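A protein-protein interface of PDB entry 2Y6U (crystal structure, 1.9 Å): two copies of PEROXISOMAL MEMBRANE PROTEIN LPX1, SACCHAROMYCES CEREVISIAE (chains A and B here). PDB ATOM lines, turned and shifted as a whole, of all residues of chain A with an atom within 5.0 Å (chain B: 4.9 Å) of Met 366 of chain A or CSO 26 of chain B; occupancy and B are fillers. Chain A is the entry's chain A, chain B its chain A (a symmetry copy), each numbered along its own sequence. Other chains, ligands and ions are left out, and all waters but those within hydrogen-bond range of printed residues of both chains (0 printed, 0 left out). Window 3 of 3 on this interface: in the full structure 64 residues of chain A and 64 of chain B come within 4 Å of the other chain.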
ATOM      1  N   PRO A 356       1.333  -0.621   6.090  1.00  0.00           N
ATOM      2  CA  PRO A 356       1.534   0.509   6.979  1.00  0.00           C
ATOM      3  C   PRO A 356       2.644   0.277   7.984  1.00  0.00           C
ATOM      4  O   PRO A 356       2.691  -0.742   8.675  1.00  0.00           O
ATOM      5  CB  PRO A 356       0.181   0.670   7.675  1.00  0.00           C
ATOM      6  CG  PRO A 356      -0.434  -0.638   7.598  1.00  0.00           C
ATOM      7  CD  PRO A 356       0.034  -1.265   6.328  1.00  0.00           C
ATOM      8  N   LEU A 358       3.317   1.970  10.868  1.00  0.00           N
ATOM      9  CA  LEU A 358       2.897   2.875  11.955  1.00  0.00           C
ATOM     10  C   LEU A 358       3.274   2.351  13.320  1.00  0.00           C
ATOM     11  O   LEU A 358       2.932   1.189  13.680  1.00  0.00           O
ATOM     12  CB  LEU A 358       1.397   3.085  11.952  1.00  0.00           C
ATOM     13  CG  LEU A 358       0.810   3.518  10.617  1.00  0.00           C
ATOM     14  CD1 LEU A 358      -0.676   3.254  10.645  1.00  0.00           C
ATOM     15  CD2 LEU A 358       1.164   5.015  10.335  1.00  0.00           C
ATOM     16  N   GLU A 362       1.311   6.335  16.743  1.00  0.00           N
ATOM     17  CA  GLU A 362       0.668   6.799  15.535  1.00  0.00           C
ATOM     18  C   GLU A 362      -0.694   6.118  15.393  1.00  0.00           C
ATOM     19  O   GLU A 362      -1.693   6.760  15.089  1.00  0.00           O
ATOM     20  CB  GLU A 362       1.524   6.475  14.342  1.00  0.00           C
ATOM     21  CG  GLU A 362       2.710   7.490  14.206  1.00  0.00           C
ATOM     22  CD  GLU A 362       3.675   7.077  13.177  1.00  0.00           C
ATOM     23  OE1 GLU A 362       3.888   5.881  12.997  1.00  0.00           O
ATOM     24  OE2 GLU A 362       4.258   7.938  12.525  1.00  0.00           O
ATOM     25  N   ARG A 363      -0.713   4.835  15.688  1.00  0.00           N
ATOM     26  CA  ARG A 363      -1.980   4.086  15.685  1.00  0.00           C
ATOM     27  C   ARG A 363      -2.990   4.662  16.666  1.00  0.00           C
ATOM     28  O   ARG A 363      -4.169   4.724  16.345  1.00  0.00           O
ATOM     29  CB  ARG A 363      -1.723   2.610  15.861  1.00  0.00           C
ATOM     30  CG  ARG A 363      -1.013   2.033  14.668  1.00  0.00           C
ATOM     31  CD  ARG A 363      -0.445   0.637  14.971  1.00  0.00           C
ATOM     32  NE  ARG A 363      -0.078  -0.124  13.781  1.00  0.00           N
ATOM     33  CZ  ARG A 363      -0.919  -0.744  12.957  1.00  0.00           C
ATOM     34  NH1 ARG A 363      -2.194  -0.808  13.237  1.00  0.00           N
ATOM     35  NH2 ARG A 363      -0.462  -1.356  11.889  1.00  0.00           N
ATOM     36  N   ALA A 364      -2.534   5.131  17.813  1.00  0.00           N
ATOM     37  CA  ALA A 364      -3.376   5.732  18.826  1.00  0.00           C
ATOM     38  C   ALA A 364      -4.059   7.026  18.343  1.00  0.00           C
ATOM     39  O   ALA A 364      -5.269   7.204  18.536  1.00  0.00           O
ATOM     40  CB  ALA A 364      -2.596   5.968  20.123  1.00  0.00           C
ATOM     41  N   VAL A 365      -3.278   7.914  17.732  1.00  0.00           N
ATOM     42  CA  VAL A 365      -3.774   9.189  17.144  1.00  0.00           C
ATOM     43  C   VAL A 365      -4.779   8.877  16.019  1.00  0.00           C
ATOM     44  O   VAL A 365      -5.833   9.476  15.944  1.00  0.00           O
ATOM     45  CB  VAL A 365      -2.592  10.008  16.576  1.00  0.00           C
ATOM     46  CG1 VAL A 365      -3.089  11.221  15.770  1.00  0.00           C
ATOM     47  CG2 VAL A 365      -1.619  10.426  17.753  1.00  0.00           C
ATOM     48  N   MET A 366      -4.451   7.920  15.177  1.00  0.00           N
ATOM     49  CA  MET A 366      -5.307   7.567  14.043  1.00  0.00           C
ATOM     50  C   MET A 366      -6.646   6.961  14.509  1.00  0.00           C
ATOM     51  O   MET A 366      -7.697   7.310  14.016  1.00  0.00           O
ATOM     52  CB  MET A 366      -4.578   6.594  13.117  1.00  0.00           C
ATOM     53  CG  MET A 366      -3.398   7.215  12.444  1.00  0.00           C
ATOM     54  SD  MET A 366      -2.171   6.005  11.968  1.00  0.00           S
ATOM     55  CE  MET A 366      -2.880   5.462  10.446  1.00  0.00           C
ATOM     56  N   PHE A 367      -6.589   6.108  15.502  1.00  0.00           N
ATOM     57  CA  PHE A 367      -7.780   5.527  16.053  1.00  0.00           C
ATOM     58  C   PHE A 367      -8.649   6.577  16.693  1.00  0.00           C
ATOM     59  O   PHE A 367      -9.871   6.561  16.523  1.00  0.00           O
ATOM     60  CB  PHE A 367      -7.502   4.454  17.112  1.00  0.00           C
ATOM     61  CG  PHE A 367      -8.706   3.957  17.711  1.00  0.00           C
ATOM     62  CD1 PHE A 367      -9.491   2.994  17.035  1.00  0.00           C
ATOM     63  CD2 PHE A 367      -9.170   4.475  18.906  1.00  0.00           C
ATOM     64  CE1 PHE A 367     -10.637   2.549  17.597  1.00  0.00           C
ATOM     65  CE2 PHE A 367     -10.327   4.033  19.453  1.00  0.00           C
ATOM     66  CZ  PHE A 367     -11.096   3.073  18.783  1.00  0.00           C
ATOM     67  N   ASP A 368      -8.045   7.419  17.511  1.00  0.00           N
ATOM     68  CA  ASP A 368      -8.822   8.416  18.204  1.00  0.00           C
ATOM     69  C   ASP A 368      -9.561   9.310  17.197  1.00  0.00           C
ATOM     70  O   ASP A 368     -10.723   9.685  17.377  1.00  0.00           O
ATOM     71  CB  ASP A 368      -7.956   9.222  19.112  1.00  0.00           C
ATOM     72  CG  ASP A 368      -7.592   8.491  20.393  1.00  0.00           C
ATOM     73  OD1 ASP A 368      -8.184   7.405  20.722  1.00  0.00           O
ATOM     74  OD2 ASP A 368      -6.707   9.060  21.125  1.00  0.00           O
ATOM     75  N   ARG A 369      -8.905   9.653  16.115  1.00  0.00           N
ATOM     76  CA  ARG A 369      -9.537  10.372  15.054  1.00  0.00           C
ATOM     77  C   ARG A 369     -10.704   9.597  14.377  1.00  0.00           C
ATOM     78  O   ARG A 369     -11.790  10.144  14.097  1.00  0.00           O
ATOM     79  CB  ARG A 369      -8.429  10.741  14.096  1.00  0.00           C
ATOM     80  CG  ARG A 369      -8.716  11.567  12.984  1.00  0.00           C
ATOM     81  CD  ARG A 369      -7.337  11.746  12.184  1.00  0.00           C
ATOM     82  NE  ARG A 369      -6.368  12.520  12.930  1.00  0.00           N
ATOM     83  CZ  ARG A 369      -5.034  12.565  12.734  1.00  0.00           C
ATOM     84  NH1 ARG A 369      -4.428  11.796  11.830  1.00  0.00           N
ATOM     85  NH2 ARG A 369      -4.287  13.378  13.500  1.00  0.00           N
ATOM     86  N   ALA A 370     -10.472   8.333  14.124  1.00  0.00           N
ATOM     87  CA  ALA A 370     -11.502   7.463  13.539  1.00  0.00           C
ATOM     88  C   ALA A 370     -12.690   7.352  14.441  1.00  0.00           C
ATOM     89  O   ALA A 370     -13.837   7.409  13.989  1.00  0.00           O
ATOM     90  CB  ALA A 370     -10.920   6.062  13.214  1.00  0.00           C
ATOM     91  N   THR B  24     -10.264  -3.391  11.735  1.00  0.00           N
ATOM     92  CA  THR B  24      -8.901  -3.042  12.098  1.00  0.00           C
ATOM     93  C   THR B  24      -8.614  -1.657  11.624  1.00  0.00           C
ATOM     94  O   THR B  24      -9.317  -1.148  10.759  1.00  0.00           O
ATOM     95  CB  THR B  24      -7.896  -4.048  11.469  1.00  0.00           C
ATOM     96  OG1 THR B  24      -8.126  -4.084  10.061  1.00  0.00           O
ATOM     97  CG2 THR B  24      -8.168  -5.461  12.002  1.00  0.00           C
ATOM     98  N   LEU B  25      -7.552  -1.059  12.149  1.00  0.00           N
ATOM     99  CA  LEU B  25      -7.136   0.260  11.752  1.00  0.00           C
ATOM    100  C   LEU B  25      -6.671   0.260  10.314  1.00  0.00           C
ATOM    101  O   LEU B  25      -7.064   1.153   9.511  1.00  0.00           O
ATOM    102  CB  LEU B  25      -6.036   0.720  12.740  1.00  0.00           C
ATOM    103  CG  LEU B  25      -5.807   2.173  12.786  1.00  0.00           C
ATOM    104  CD1 LEU B  25      -7.138   2.774  13.343  1.00  0.00           C
ATOM    105  CD2 LEU B  25      -4.606   2.457  13.661  1.00  0.00           C
ATOM    106  N   CSO B  26      -5.831  -0.722   9.967  1.00  0.00           N
ATOM    107  CA  CSO B  26      -5.345  -0.881   8.608  1.00  0.00           C
ATOM    108  CB  CSO B  26      -3.804  -0.764   8.579  1.00  0.00           C
ATOM    109  SG  CSO B  26      -3.155   0.673   9.498  1.00  0.00           S
ATOM    110  C   CSO B  26      -5.729  -2.225   7.998  1.00  0.00           C
ATOM    111  O   CSO B  26      -5.920  -3.224   8.724  1.00  0.00           O
ATOM    112  OD  CSO B  26      -3.711   2.117   8.447  1.00  0.00           O
ATOM    113  N   ALA B  27      -5.838  -2.283   6.673  1.00  0.00           N
ATOM    114  CA  ALA B  27      -6.427  -3.505   6.062  1.00  0.00           C
ATOM    115  C   ALA B  27      -5.457  -4.648   6.204  1.00  0.00           C
ATOM    116  O   ALA B  27      -5.908  -5.808   6.238  1.00  0.00           O
ATOM    117  CB  ALA B  27      -6.801  -3.310   4.546  1.00  0.00           C
ATOM    118  N   THR B  28      -4.179  -4.352   6.323  1.00  0.00           N
ATOM    119  CA  THR B  28      -3.205  -5.399   6.566  1.00  0.00           C
ATOM    120  C   THR B  28      -2.995  -5.862   7.986  1.00  0.00           C
ATOM    121  O   THR B  28      -2.218  -6.793   8.205  1.00  0.00           O
ATOM    122  CB  THR B  28      -1.882  -5.036   6.023  1.00  0.00           C
ATOM    123  OG1 THR B  28      -1.412  -3.830   6.661  1.00  0.00           O
ATOM    124  CG2 THR B  28      -2.001  -4.861   4.467  1.00  0.00           C
ATOM    125  N   ASP B  29      -3.675  -5.239   8.956  1.00  0.00           N
ATOM    126  CA  ASP B  29      -3.589  -5.700  10.362  1.00  0.00           C
ATOM    127  C   ASP B  29      -4.273  -7.043  10.512  1.00  0.00           C
ATOM    128  O   ASP B  29      -5.222  -7.305   9.812  1.00  0.00           O
ATOM    129  CB  ASP B  29      -4.314  -4.740  11.251  1.00  0.00           C
ATOM    130  CG  ASP B  29      -3.528  -3.383  11.401  1.00  0.00           C
ATOM    131  OD1 ASP B  29      -2.287  -3.290  11.162  1.00  0.00           O
ATOM    132  OD2 ASP B  29      -4.210  -2.403  11.733  1.00  0.00           O
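Of the printed residues of chain B, Leu 358 of chain A touches CSO 26. Glu 362 of chain A touches none of the printed residues of chain B. Printed residues of chain B within 4 Å of Arg 363 of chain A: Leu 25 (3.5 Å) and Asp 29 (2.8 Å). Printed residues of chain B within 4 Å of Met 366 of chain A: CSO 26 (3.98 Å). Of the printed residues of chain B, Phe 367 of chain A touches Leu 25 (3.9 Å). Of the printed residues of chain A, CSO 26 of chain B touches Pro 356, Leu 358 and Met 366. Ala 27 of chain B touches none of the printed residues of chain A. The nearest printed residue of chain B that does not touch Met 366 of chain A is Leu 25 of chain B (4.2 Å).
Of the 11 printed residues of chain A, 5 touch a printed residue of chain B. Printed residues of chain A that touch a printed residue of chain B: Pro 356, Leu 358, Arg 363, Met 366 and Phe 367. Hydrophobic or aromatic side chains of chain A within 4 Å of the printed part of chain B: Pro 356, Leu 358 and Met 366. Printed residues of chain B that touch a printed residue of chain A: Leu 25, CSO 26, Thr 28 and Asp 29. Hydrophobic or aromatic side chains of chain B within 4 Å of the printed part of chain A: Leu 25.
The backbone carbonyl oxygen (O) of Leu 358 of chain A is in hydrogen-bond range of the guanidinium group (NE) of Arg 363 of chain A (3.3 Å). The side-chain hydroxyl of Thr 24 of chain B is in hydrogen-bond range of O of CSO 26 of chain B (2.7 Å). OD2 of Asp 29 of chain B lies within hydrogen-bond range of N of CSO 26 of chain B (2.9 Å).
NH2 of Arg 363 of chain A lies within salt-bridge range of OD1 of Asp 29 of chain B (2.8 Å).
No position is printed for both chains.
Among the printed residues, pairs that only touch across the chains: Pro 356 of chain A with Thr 28 of chain B, Pro 356 of chain A with CSO 26 of chain B, Arg 363 of chain A with Leu 25 of chain B, Leu 358 of chain A with CSO 26 of chain B, Phe 367 of chain A with Leu 25 of chain B and Met 366 of chain A with CSO 26 of chain B.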
